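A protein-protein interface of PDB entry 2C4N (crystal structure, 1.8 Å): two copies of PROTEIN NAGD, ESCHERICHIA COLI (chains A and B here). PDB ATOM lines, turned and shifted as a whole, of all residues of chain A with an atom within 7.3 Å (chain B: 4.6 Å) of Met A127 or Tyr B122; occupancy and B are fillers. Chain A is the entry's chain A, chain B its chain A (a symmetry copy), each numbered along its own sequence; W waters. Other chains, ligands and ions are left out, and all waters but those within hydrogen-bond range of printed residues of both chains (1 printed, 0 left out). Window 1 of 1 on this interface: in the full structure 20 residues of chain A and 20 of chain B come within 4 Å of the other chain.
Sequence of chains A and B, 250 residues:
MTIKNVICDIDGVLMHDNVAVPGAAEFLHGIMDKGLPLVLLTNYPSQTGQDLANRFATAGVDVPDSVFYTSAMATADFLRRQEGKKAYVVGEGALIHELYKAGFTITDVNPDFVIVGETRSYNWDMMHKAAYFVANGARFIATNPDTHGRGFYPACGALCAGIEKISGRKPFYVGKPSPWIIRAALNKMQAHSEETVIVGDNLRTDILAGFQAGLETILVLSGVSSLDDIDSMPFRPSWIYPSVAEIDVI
Water W1 lies within hydrogen-bond range of OD2 of Asp A125 (2.7 Å), O of Arg B120 (2.9 Å) and N of Trp A124 (3.5 Å).
Asn B123 touches Tyr A122.
CE2 of Tyr A122 touches CE of Met B127 (3.6 Å).
O of Tyr B122 touches CA of Asn A123, at 3.2 Å.
Asn B123 touches Asn A123 (CA to CA, 3.99 Å).
Thr B119 touches Trp A124 (O to CD1, 3.2 Å).
O of Arg B120 touches CB of Trp A124, at 3.2 Å.
Tyr B122 touches Met A127.
CB of His A128 touches CD of Pro B154 (3.6 Å).
Gly A162 touches Ala B158.
Ile A166 touches Ala B158 (CG1 to CB, 3.6 Å).
N of Trp A124 sits at hydrogen-bond distance from O of Tyr B122 (2.9 Å).
The backbone carbonyl oxygen (O) of Pro B154 sits at hydrogen-bond distance from the indole nitrogen (NE1) of Trp A124, 3.3 Å away.
Hydrophobic or aromatic side chains of chain A within 4 Å of the printed part of chain B: Tyr A122, Trp A124, Met A127, His A128, Ala A158 and Ile A166.
Among the printed residues, no Asp or Glu carboxylate lies within 4 Å of a Lys or Arg side-chain nitrogen of the other chain.
Tyr A122 touches Asn B123, and with the chains exchanged Asn A123 touches Tyr B122.
Tyr A122 touches Met B127, and with the chains exchanged Met A127 touches Tyr B122.
Asn B123 touches its own counterpart, Asn A123.
Met A127 touches Ala B158, and with the chains exchanged Ala A158 touches Met B127.
9 positions are printed for both chains.
OH of Tyr A122 lies within hydrogen-bond range of O of Leu A159 (2.8 Å).
OD1 of Asn A123 is in hydrogen-bond range of N of Asp A125.
N of Met A126 is in hydrogen-bond range of OD1 of Asn A123 (2.9 Å).
OG1 of Thr B119 sits close to N of Ser B121 (3.1 Å).
OH of Tyr B122 lies within hydrogen-bond range of O of Leu B159.
OD1 of Asn B123 lies within hydrogen-bond range of N of Met B126 (2.9 Å).
Of the printed residues of chain B, Tyr A122 touches Asn B123 and Met B127.
Of the printed residues of chain B, His A128 touches Pro B154 (3.6 Å).
Phe A133 touches none of the printed residues of chain B.
Of the printed residues of chain B, Gly A162 touches Ala B158.
Ile A163 touches none of the printed residues of chain B.
Of chain A, only Asn A123, Trp A124 and Met A127 come within 4 Å of Tyr B122.
Printed residues of chain A within 4 Å of Asn B123: Tyr A122 (3.2 Å) and Asn A123 (3.99 Å).
Of the printed residues of chain A, Pro B154 touches Trp A124, Met A127, His A128 and Ile A166.
The nearest residue of chain B that does not touch Met A127 is Leu B159 (4.3 Å).
The nearest printed residue of chain B that does not touch Asn A123 is Ser B121 (5.3 Å).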
ATOM      1  N   TYR A  88     -14.297  -5.613  22.773  1.00  0.00           N
ATOM      2  CA  TYR A  88     -14.355  -4.184  22.541  1.00  0.00           C
ATOM      3  C   TYR A  88     -12.907  -3.799  22.822  1.00  0.00           C
ATOM      4  O   TYR A  88     -12.394  -4.043  23.919  1.00  0.00           O
ATOM      5  CB  TYR A  88     -15.296  -3.481  23.521  1.00  0.00           C
ATOM      6  CG  TYR A  88     -15.213  -1.981  23.396  1.00  0.00           C
ATOM      7  CD1 TYR A  88     -14.623  -1.209  24.397  1.00  0.00           C
ATOM      8  CD2 TYR A  88     -15.657  -1.336  22.243  1.00  0.00           C
ATOM      9  CE1 TYR A  88     -14.472   0.167  24.251  1.00  0.00           C
ATOM     10  CE2 TYR A  88     -15.509   0.041  22.084  1.00  0.00           C
ATOM     11  CZ  TYR A  88     -14.914   0.786  23.091  1.00  0.00           C
ATOM     12  OH  TYR A  88     -14.747   2.143  22.928  1.00  0.00           O
ATOM     13  N   VAL A  90      -9.759  -0.998  23.023  1.00  0.00           N
ATOM     14  CA  VAL A  90      -9.328   0.381  23.188  1.00  0.00           C
ATOM     15  C   VAL A  90      -7.857   0.299  22.808  1.00  0.00           C
ATOM     16  O   VAL A  90      -6.999   0.029  23.640  1.00  0.00           O
ATOM     17  CB  VAL A  90      -9.461   0.856  24.652  1.00  0.00           C
ATOM     18  CG1 VAL A  90      -8.889   2.263  24.799  1.00  0.00           C
ATOM     19  CG2 VAL A  90     -10.927   0.840  25.077  1.00  0.00           C
ATOM     20  N   SER A 121      -5.941   7.979  20.130  1.00  0.00           N
ATOM     21  CA  SER A 121      -7.304   8.393  19.817  1.00  0.00           C
ATOM     22  C   SER A 121      -8.207   8.178  21.023  1.00  0.00           C
ATOM     23  O   SER A 121      -9.408   8.434  20.960  1.00  0.00           O
ATOM     24  CB  SER A 121      -7.850   7.604  18.625  1.00  0.00           C
ATOM     25  OG  SER A 121      -7.225   8.013  17.420  1.00  0.00           O
ATOM     26  N   TYR A 122      -7.622   7.698  22.116  1.00  0.00           N
ATOM     27  CA  TYR A 122      -8.369   7.449  23.349  1.00  0.00           C
ATOM     28  C   TYR A 122      -9.198   8.682  23.697  1.00  0.00           C
ATOM     29  O   TYR A 122      -8.685   9.805  23.683  1.00  0.00           O
ATOM     30  CB  TYR A 122      -7.404   7.161  24.500  1.00  0.00           C
ATOM     31  CG  TYR A 122      -8.067   6.812  25.821  1.00  0.00           C
ATOM     32  CD1 TYR A 122      -8.734   5.603  25.991  1.00  0.00           C
ATOM     33  CD2 TYR A 122      -7.982   7.672  26.916  1.00  0.00           C
ATOM     34  CE1 TYR A 122      -9.299   5.251  27.227  1.00  0.00           C
ATOM     35  CE2 TYR A 122      -8.540   7.331  28.151  1.00  0.00           C
ATOM     36  CZ  TYR A 122      -9.194   6.120  28.298  1.00  0.00           C
ATOM     37  OH  TYR A 122      -9.739   5.779  29.515  1.00  0.00           O
ATOM     38  N   ASN A 123     -10.473   8.476  24.015  1.00  0.00           N
ATOM     39  CA  ASN A 123     -11.336   9.594  24.370  1.00  0.00           C
ATOM     40  C   ASN A 123     -12.437   9.216  25.350  1.00  0.00           C
ATOM     41  O   ASN A 123     -12.558   8.063  25.766  1.00  0.00           O
ATOM     42  CB  ASN A 123     -11.958  10.219  23.107  1.00  0.00           C
ATOM     43  CG  ASN A 123     -12.817   9.242  22.327  1.00  0.00           C
ATOM     44  OD1 ASN A 123     -13.333   8.271  22.876  1.00  0.00           O
ATOM     45  ND2 ASN A 123     -12.985   9.508  21.036  1.00  0.00           N
ATOM     46  N   TRP A 124     -13.233  10.217  25.706  1.00  0.00           N
ATOM     47  CA  TRP A 124     -14.351  10.084  26.630  1.00  0.00           C
ATOM     48  C   TRP A 124     -15.280   8.929  26.251  1.00  0.00           C
ATOM     49  O   TRP A 124     -15.715   8.159  27.107  1.00  0.00           O
ATOM     50  CB  TRP A 124     -15.132  11.402  26.639  1.00  0.00           C
ATOM     51  CG  TRP A 124     -16.106  11.563  27.764  1.00  0.00           C
ATOM     52  CD1 TRP A 124     -15.881  12.175  28.963  1.00  0.00           C
ATOM     53  CD2 TRP A 124     -17.478  11.149  27.777  1.00  0.00           C
ATOM     54  NE1 TRP A 124     -17.028  12.173  29.719  1.00  0.00           N
ATOM     55  CE2 TRP A 124     -18.023  11.543  29.017  1.00  0.00           C
ATOM     56  CE3 TRP A 124     -18.298  10.476  26.862  1.00  0.00           C
ATOM     57  CZ2 TRP A 124     -19.359  11.297  29.363  1.00  0.00           C
ATOM     58  CZ3 TRP A 124     -19.627  10.230  27.206  1.00  0.00           C
ATOM     59  CH2 TRP A 124     -20.141  10.636  28.448  1.00  0.00           C
ATOM     60  N   ASP A 125     -15.588   8.816  24.964  1.00  0.00           N
ATOM     61  CA  ASP A 125     -16.471   7.751  24.496  1.00  0.00           C
ATOM     62  C   ASP A 125     -15.911   6.352  24.745  1.00  0.00           C
ATOM     63  O   ASP A 125     -16.635   5.460  25.179  1.00  0.00           O
ATOM     64  CB  ASP A 125     -16.780   7.934  23.006  1.00  0.00           C
ATOM     65  CG  ASP A 125     -17.619   9.169  22.736  1.00  0.00           C
ATOM     66  OD1 ASP A 125     -18.717   9.283  23.324  1.00  0.00           O
ATOM     67  OD2 ASP A 125     -17.183  10.021  21.933  1.00  0.00           O
ATOM     68  N   MET A 126     -14.629   6.160  24.467  1.00  0.00           N
ATOM     69  CA  MET A 126     -13.991   4.865  24.684  1.00  0.00           C
ATOM     70  C   MET A 126     -13.964   4.521  26.166  1.00  0.00           C
ATOM     71  O   MET A 126     -14.244   3.393  26.555  1.00  0.00           O
ATOM     72  CB  MET A 126     -12.561   4.877  24.141  1.00  0.00           C
ATOM     73  CG  MET A 126     -12.462   4.907  22.627  1.00  0.00           C
ATOM     74  SD  MET A 126     -10.750   4.742  22.102  1.00  0.00           S
ATOM     75  CE  MET A 126     -10.771   5.648  20.556  1.00  0.00           C
ATOM     76  N   MET A 127     -13.620   5.500  26.995  1.00  0.00           N
ATOM     77  CA  MET A 127     -13.572   5.274  28.437  1.00  0.00           C
ATOM     78  C   MET A 127     -14.960   4.874  28.921  1.00  0.00           C
ATOM     79  O   MET A 127     -15.113   3.957  29.726  1.00  0.00           O
ATOM     80  CB  MET A 127     -13.124   6.544  29.167  1.00  0.00           C
ATOM     81  CG  MET A 127     -12.859   6.334  30.649  1.00  0.00           C
ATOM     82  SD  MET A 127     -12.667   7.852  31.604  1.00  0.00           S
ATOM     83  CE  MET A 127     -11.238   8.585  30.839  1.00  0.00           C
ATOM     84  N   HIS A 128     -15.968   5.575  28.412  1.00  0.00           N
ATOM     85  CA  HIS A 128     -17.359   5.322  28.768  1.00  0.00           C
ATOM     86  C   HIS A 128     -17.781   3.899  28.414  1.00  0.00           C
ATOM     87  O   HIS A 128     -18.255   3.152  29.267  1.00  0.00           O
ATOM     88  CB  HIS A 128     -18.267   6.327  28.047  1.00  0.00           C
ATOM     89  CG  HIS A 128     -19.730   6.051  28.211  1.00  0.00           C
ATOM     90  ND1 HIS A 128     -20.644   6.283  27.205  1.00  0.00           N
ATOM     91  CD2 HIS A 128     -20.438   5.574  29.260  1.00  0.00           C
ATOM     92  CE1 HIS A 128     -21.853   5.956  27.628  1.00  0.00           C
ATOM     93  NE2 HIS A 128     -21.755   5.523  28.872  1.00  0.00           N
ATOM     94  N   LYS A 129     -17.612   3.526  27.150  1.00  0.00           N
ATOM     95  CA  LYS A 129     -17.995   2.189  26.707  1.00  0.00           C
ATOM     96  C   LYS A 129     -17.232   1.092  27.429  1.00  0.00           C
ATOM     97  O   LYS A 129     -17.822   0.104  27.862  1.00  0.00           O
ATOM     98  CB  LYS A 129     -17.790   2.039  25.200  1.00  0.00           C
ATOM     99  CG  LYS A 129     -18.701   2.903  24.345  1.00  0.00           C
ATOM    100  CD  LYS A 129     -18.592   2.474  22.888  1.00  0.00           C
ATOM    101  CE  LYS A 129     -19.258   3.455  21.944  1.00  0.00           C
ATOM    102  NZ  LYS A 129     -19.085   3.021  20.524  1.00  0.00           N
ATOM    103  N   ALA A 130     -15.921   1.259  27.552  1.00  0.00           N
ATOM    104  CA  ALA A 130     -15.101   0.263  28.234  1.00  0.00           C
ATOM    105  C   ALA A 130     -15.573   0.095  29.674  1.00  0.00           C
ATOM    106  O   ALA A 130     -15.725  -1.022  30.160  1.00  0.00           O
ATOM    107  CB  ALA A 130     -13.626   0.684  28.204  1.00  0.00           C
ATOM    108  N   ALA A 131     -15.823   1.215  30.347  1.00  0.00           N
ATOM    109  CA  ALA A 131     -16.277   1.176  31.734  1.00  0.00           C
ATOM    110  C   ALA A 131     -17.641   0.493  31.831  1.00  0.00           C
ATOM    111  O   ALA A 131     -17.881  -0.306  32.732  1.00  0.00           O
ATOM    112  CB  ALA A 131     -16.354   2.595  32.302  1.00  0.00           C
ATOM    113  N   TYR A 132     -18.525   0.815  30.894  1.00  0.00           N
ATOM    114  CA  TYR A 132     -19.859   0.225  30.858  1.00  0.00           C
ATOM    115  C   TYR A 132     -19.783  -1.296  30.709  1.00  0.00           C
ATOM    116  O   TYR A 132     -20.443  -2.032  31.444  1.00  0.00           O
ATOM    117  CB  TYR A 132     -20.652   0.815  29.693  1.00  0.00           C
ATOM    118  CG  TYR A 132     -21.989   0.148  29.461  1.00  0.00           C
ATOM    119  CD1 TYR A 132     -23.095   0.456  30.252  1.00  0.00           C
ATOM    120  CD2 TYR A 132     -22.144  -0.802  28.453  1.00  0.00           C
ATOM    121  CE1 TYR A 132     -24.327  -0.167  30.045  1.00  0.00           C
ATOM    122  CE2 TYR A 132     -23.368  -1.431  28.237  1.00  0.00           C
ATOM    123  CZ  TYR A 132     -24.453  -1.109  29.035  1.00  0.00           C
ATOM    124  OH  TYR A 132     -25.663  -1.729  28.819  1.00  0.00           O
ATOM    125  N   PHE A 133     -18.982  -1.767  29.757  1.00  0.00           N
ATOM    126  CA  PHE A 133     -18.846  -3.206  29.537  1.00  0.00           C
ATOM    127  C   PHE A 133     -18.197  -3.931  30.715  1.00  0.00           C
ATOM    128  O   PHE A 133     -18.645  -5.007  31.116  1.00  0.00           O
ATOM    129  CB  PHE A 133     -18.047  -3.483  28.261  1.00  0.00           C
ATOM    130  CG  PHE A 133     -18.741  -3.042  27.000  1.00  0.00           C
ATOM    131  CD1 PHE A 133     -20.061  -3.411  26.753  1.00  0.00           C
ATOM    132  CD2 PHE A 133     -18.072  -2.266  26.054  1.00  0.00           C
ATOM    133  CE1 PHE A 133     -20.707  -3.012  25.581  1.00  0.00           C
ATOM    134  CE2 PHE A 133     -18.709  -1.862  24.877  1.00  0.00           C
ATOM    135  CZ  PHE A 133     -20.031  -2.238  24.642  1.00  0.00           C
ATOM    136  N   ALA A 158      -2.358   4.272  31.996  1.00  0.00           N
ATOM    137  CA  ALA A 158      -3.072   5.539  32.137  1.00  0.00           C
ATOM    138  C   ALA A 158      -4.463   5.470  31.505  1.00  0.00           C
ATOM    139  O   ALA A 158      -5.411   6.086  31.997  1.00  0.00           O
ATOM    140  CB  ALA A 158      -2.259   6.667  31.503  1.00  0.00           C
ATOM    141  N   LEU A 159      -4.579   4.726  30.410  1.00  0.00           N
ATOM    142  CA  LEU A 159      -5.861   4.574  29.733  1.00  0.00           C
ATOM    143  C   LEU A 159      -6.799   3.721  30.578  1.00  0.00           C
ATOM    144  O   LEU A 159      -8.014   3.909  30.561  1.00  0.00           O
ATOM    145  CB  LEU A 159      -5.678   3.926  28.353  1.00  0.00           C
ATOM    146  CG  LEU A 159      -4.676   4.586  27.388  1.00  0.00           C
ATOM    147  CD1 LEU A 159      -4.902   4.037  25.986  1.00  0.00           C
ATOM    148  CD2 LEU A 159      -4.851   6.090  27.390  1.00  0.00           C
ATOM    149  N   CYS A 160      -6.240   2.777  31.324  1.00  0.00           N
ATOM    150  CA  CYS A 160      -7.059   1.918  32.177  1.00  0.00           C
ATOM    151  C   CYS A 160      -7.562   2.640  33.420  1.00  0.00           C
ATOM    152  O   CYS A 160      -8.639   2.335  33.933  1.00  0.00           O
ATOM    153  CB  CYS A 160      -6.261   0.683  32.613  1.00  0.00           C
ATOM    154  SG  CYS A 160      -5.956  -0.527  31.302  1.00  0.00           S
ATOM    155  N   ALA A 161      -6.780   3.603  33.895  1.00  0.00           N
ATOM    156  CA  ALA A 161      -7.113   4.344  35.108  1.00  0.00           C
ATOM    157  C   ALA A 161      -8.562   4.836  35.199  1.00  0.00           C
ATOM    158  O   ALA A 161      -9.242   4.597  36.203  1.00  0.00           O
ATOM    159  CB  ALA A 161      -6.143   5.515  35.274  1.00  0.00           C
ATOM    160  N   GLY A 162      -9.031   5.523  34.161  1.00  0.00           N
ATOM    161  CA  GLY A 162     -10.397   6.022  34.163  1.00  0.00           C
ATOM    162  C   GLY A 162     -11.426   4.905  34.134  1.00  0.00           C
ATOM    163  O   GLY A 162     -12.461   4.980  34.795  1.00  0.00           O
ATOM    164  N   ILE A 163     -11.139   3.864  33.359  1.00  0.00           N
ATOM    165  CA  ILE A 163     -12.038   2.720  33.250  1.00  0.00           C
ATOM    166  C   ILE A 163     -12.162   2.006  34.595  1.00  0.00           C
ATOM    167  O   ILE A 163     -13.257   1.619  35.001  1.00  0.00           O
ATOM    168  CB  ILE A 163     -11.529   1.726  32.177  1.00  0.00           C
ATOM    169  CG1 ILE A 163     -11.495   2.426  30.811  1.00  0.00           C
ATOM    170  CG2 ILE A 163     -12.427   0.496  32.126  1.00  0.00           C
ATOM    171  CD1 ILE A 163     -10.653   1.712  29.763  1.00  0.00           C
ATOM    172  N   GLU A 164     -11.037   1.841  35.285  1.00  0.00           N
ATOM    173  CA  GLU A 164     -11.023   1.187  36.595  1.00  0.00           C
ATOM    174  C   GLU A 164     -11.792   2.020  37.620  1.00  0.00           C
ATOM    175  O   GLU A 164     -12.554   1.486  38.426  1.00  0.00           O
ATOM    176  CB  GLU A 164      -9.581   1.007  37.093  1.00  0.00           C
ATOM    177  CG  GLU A 164      -8.689   0.199  36.174  1.00  0.00           C
ATOM    178  CD  GLU A 164      -7.268   0.084  36.686  1.00  0.00           C
ATOM    179  OE1 GLU A 164      -7.048  -0.596  37.707  1.00  0.00           O
ATOM    180  OE2 GLU A 164      -6.363   0.679  36.069  1.00  0.00           O
ATOM    181  N   LYS A 165     -11.579   3.330  37.582  1.00  0.00           N
ATOM    182  CA  LYS A 165     -12.232   4.261  38.506  1.00  0.00           C
ATOM    183  C   LYS A 165     -13.757   4.195  38.412  1.00  0.00           C
ATOM    184  O   LYS A 165     -14.453   4.153  39.426  1.00  0.00           O
ATOM    185  CB  LYS A 165     -11.772   5.690  38.207  1.00  0.00           C
ATOM    186  CG  LYS A 165     -11.461   6.531  39.432  1.00  0.00           C
ATOM    187  CD  LYS A 165     -10.312   5.915  40.212  1.00  0.00           C
ATOM    188  CE  LYS A 165      -9.440   6.976  40.866  1.00  0.00           C
ATOM    189  NZ  LYS A 165      -8.151   6.412  41.367  1.00  0.00           N
ATOM    190  N   ILE A 166     -14.263   4.179  37.185  1.00  0.00           N
ATOM    191  CA  ILE A 166     -15.702   4.133  36.943  1.00  0.00           C
ATOM    192  C   ILE A 166     -16.317   2.768  37.235  1.00  0.00           C
ATOM    193  O   ILE A 166     -17.355   2.678  37.891  1.00  0.00           O
ATOM    194  CB  ILE A 166     -16.027   4.509  35.475  1.00  0.00           C
ATOM    195  CG1 ILE A 166     -15.549   5.934  35.187  1.00  0.00           C
ATOM    196  CG2 ILE A 166     -17.535   4.389  35.216  1.00  0.00           C
ATOM    197  CD1 ILE A 166     -15.626   6.331  33.724  1.00  0.00           C
ATOM    198  N   VAL B  90      -9.196  21.350  31.391  1.00  0.00           N
ATOM    199  CA  VAL B  90      -9.731  20.131  30.808  1.00  0.00           C
ATOM    200  C   VAL B  90     -11.195  20.201  31.217  1.00  0.00           C
ATOM    201  O   VAL B  90     -11.578  19.746  32.289  1.00  0.00           O
ATOM    202  CB  VAL B  90      -9.082  18.867  31.415  1.00  0.00           C
ATOM    203  CG1 VAL B  90      -9.756  17.615  30.860  1.00  0.00           C
ATOM    204  CG2 VAL B  90      -7.589  18.842  31.098  1.00  0.00           C
ATOM    205  N   THR B 119     -15.757  17.098  30.453  1.00  0.00           N
ATOM    206  CA  THR B 119     -15.858  17.392  29.034  1.00  0.00           C
ATOM    207  C   THR B 119     -15.908  16.087  28.264  1.00  0.00           C
ATOM    208  O   THR B 119     -15.064  15.215  28.451  1.00  0.00           O
ATOM    209  CB  THR B 119     -14.674  18.240  28.525  1.00  0.00           C
ATOM    210  OG1 THR B 119     -14.758  18.351  27.097  1.00  0.00           O
ATOM    211  CG2 THR B 119     -13.341  17.606  28.911  1.00  0.00           C
ATOM    212  N   ARG B 120     -16.915  15.949  27.411  1.00  0.00           N
ATOM    213  CA  ARG B 120     -17.060  14.739  26.622  1.00  0.00           C
ATOM    214  C   ARG B 120     -16.055  14.712  25.486  1.00  0.00           C
ATOM    215  O   ARG B 120     -16.040  13.778  24.689  1.00  0.00           O
ATOM    216  CB  ARG B 120     -18.471  14.638  26.050  1.00  0.00           C
ATOM    217  CG  ARG B 120     -19.579  14.505  27.077  1.00  0.00           C
ATOM    218  CD  ARG B 120     -20.834  14.069  26.357  1.00  0.00           C
ATOM    219  NE  ARG B 120     -21.943  13.746  27.246  1.00  0.00           N
ATOM    220  CZ  ARG B 120     -23.011  13.056  26.863  1.00  0.00           C
ATOM    221  NH1 ARG B 120     -23.102  12.620  25.614  1.00  0.00           N
ATOM    222  NH2 ARG B 120     -23.989  12.804  27.720  1.00  0.00           N
ATOM    223  N   SER B 121     -15.229  15.753  25.407  1.00  0.00           N
ATOM    224  CA  SER B 121     -14.202  15.850  24.377  1.00  0.00           C
ATOM    225  C   SER B 121     -12.859  15.395  24.931  1.00  0.00           C
ATOM    226  O   SER B 121     -11.848  15.429  24.231  1.00  0.00           O
ATOM    227  CB  SER B 121     -14.080  17.287  23.866  1.00  0.00           C
ATOM    228  OG  SER B 121     -15.203  17.638  23.075  1.00  0.00           O
ATOM    229  N   TYR B 122     -12.857  14.978  26.193  1.00  0.00           N
ATOM    230  CA  TYR B 122     -11.638  14.507  26.852  1.00  0.00           C
ATOM    231  C   TYR B 122     -10.944  13.481  25.960  1.00  0.00           C
ATOM    232  O   TYR B 122     -11.587  12.556  25.454  1.00  0.00           O
ATOM    233  CB  TYR B 122     -11.982  13.847  28.188  1.00  0.00           C
ATOM    234  CG  TYR B 122     -10.786  13.384  29.001  1.00  0.00           C
ATOM    235  CD1 TYR B 122      -9.928  14.301  29.601  1.00  0.00           C
ATOM    236  CD2 TYR B 122     -10.545  12.027  29.213  1.00  0.00           C
ATOM    237  CE1 TYR B 122      -8.855  13.878  30.400  1.00  0.00           C
ATOM    238  CE2 TYR B 122      -9.480  11.595  30.009  1.00  0.00           C
ATOM    239  CZ  TYR B 122      -8.643  12.525  30.599  1.00  0.00           C
ATOM    240  OH  TYR B 122      -7.597  12.103  31.388  1.00  0.00           O
ATOM    241  N   ASN B 123      -9.637  13.637  25.772  1.00  0.00           N
ATOM    242  CA  ASN B 123      -8.892  12.700  24.942  1.00  0.00           C
ATOM    243  C   ASN B 123      -7.440  12.542  25.369  1.00  0.00           C
ATOM    244  O   ASN B 123      -6.978  13.175  26.320  1.00  0.00           O
ATOM    245  CB  ASN B 123      -8.955  13.119  23.462  1.00  0.00           C
ATOM    246  CG  ASN B 123      -8.353  14.489  23.211  1.00  0.00           C
ATOM    247  OD1 ASN B 123      -7.511  14.962  23.970  1.00  0.00           O
ATOM    248  ND2 ASN B 123      -8.778  15.128  22.125  1.00  0.00           N
ATOM    249  N   MET B 126      -5.358  15.766  25.811  1.00  0.00           N
ATOM    250  CA  MET B 126      -5.637  16.513  27.034  1.00  0.00           C
ATOM    251  C   MET B 126      -4.994  15.836  28.235  1.00  0.00           C
ATOM    252  O   MET B 126      -4.405  16.492  29.087  1.00  0.00           O
ATOM    253  CB  MET B 126      -7.145  16.622  27.261  1.00  0.00           C
ATOM    254  CG  MET B 126      -7.865  17.538  26.288  1.00  0.00           C
ATOM    255  SD  MET B 126      -9.591  17.726  26.755  1.00  0.00           S
ATOM    256  CE  MET B 126     -10.354  18.015  25.161  1.00  0.00           C
ATOM    257  N   MET B 127      -5.115  14.515  28.304  1.00  0.00           N
ATOM    258  CA  MET B 127      -4.526  13.770  29.414  1.00  0.00           C
ATOM    259  C   MET B 127      -3.018  13.987  29.411  1.00  0.00           C
ATOM    260  O   MET B 127      -2.403  14.200  30.454  1.00  0.00           O
ATOM    261  CB  MET B 127      -4.825  12.274  29.278  1.00  0.00           C
ATOM    262  CG  MET B 127      -4.418  11.457  30.493  1.00  0.00           C
ATOM    263  SD  MET B 127      -4.433   9.670  30.242  1.00  0.00           S
ATOM    264  CE  MET B 127      -6.147   9.371  29.868  1.00  0.00           C
ATOM    265  N   PRO B 154     -18.339   9.020  32.228  1.00  0.00           N
ATOM    266  CA  PRO B 154     -17.166   9.525  32.943  1.00  0.00           C
ATOM    267  C   PRO B 154     -17.432  10.916  33.512  1.00  0.00           C
ATOM    268  O   PRO B 154     -18.058  11.754  32.856  1.00  0.00           O
ATOM    269  CB  PRO B 154     -16.086   9.544  31.861  1.00  0.00           C
ATOM    270  CG  PRO B 154     -16.489   8.392  30.967  1.00  0.00           C
ATOM    271  CD  PRO B 154     -17.984   8.602  30.861  1.00  0.00           C
ATOM    272  N   ALA B 158     -12.954  10.521  37.019  1.00  0.00           N
ATOM    273  CA  ALA B 158     -12.455   9.582  36.017  1.00  0.00           C
ATOM    274  C   ALA B 158     -11.458  10.252  35.071  1.00  0.00           C
ATOM    275  O   ALA B 158     -10.501   9.623  34.613  1.00  0.00           O
ATOM    276  CB  ALA B 158     -13.624   8.997  35.226  1.00  0.00           C
ATOM    277  N   LEU B 159     -11.689  11.526  34.773  1.00  0.00           N
ATOM    278  CA  LEU B 159     -10.795  12.271  33.894  1.00  0.00           C
ATOM    279  C   LEU B 159      -9.470  12.533  34.599  1.00  0.00           C
ATOM    280  O   LEU B 159      -8.417  12.592  33.967  1.00  0.00           O
ATOM    281  CB  LEU B 159     -11.428  13.604  33.473  1.00  0.00           C
ATOM    282  CG  LEU B 159     -12.829  13.553  32.836  1.00  0.00           C
ATOM    283  CD1 LEU B 159     -13.119  14.891  32.169  1.00  0.00           C
ATOM    284  CD2 LEU B 159     -12.908  12.437  31.817  1.00  0.00           C
ATOM    285  N   ILE B 163      -4.450  11.354  34.542  1.00  0.00           N
ATOM    286  CA  ILE B 163      -3.510  12.433  34.820  1.00  0.00           C
ATOM    287  C   ILE B 163      -2.730  12.147  36.102  1.00  0.00           C
ATOM    288  O   ILE B 163      -1.519  12.357  36.160  1.00  0.00           O
ATOM    289  CB  ILE B 163      -4.253  13.786  34.952  1.00  0.00           C
ATOM    290  CG1 ILE B 163      -4.958  14.110  33.628  1.00  0.00           C
ATOM    291  CG2 ILE B 163      -3.276  14.894  35.324  1.00  0.00           C
ATOM    292  CD1 ILE B 163      -6.035  15.180  33.738  1.00  0.00           C
HETATM  293  O   HOH W   1     -15.196  11.484  23.144  1.00  0.00           O
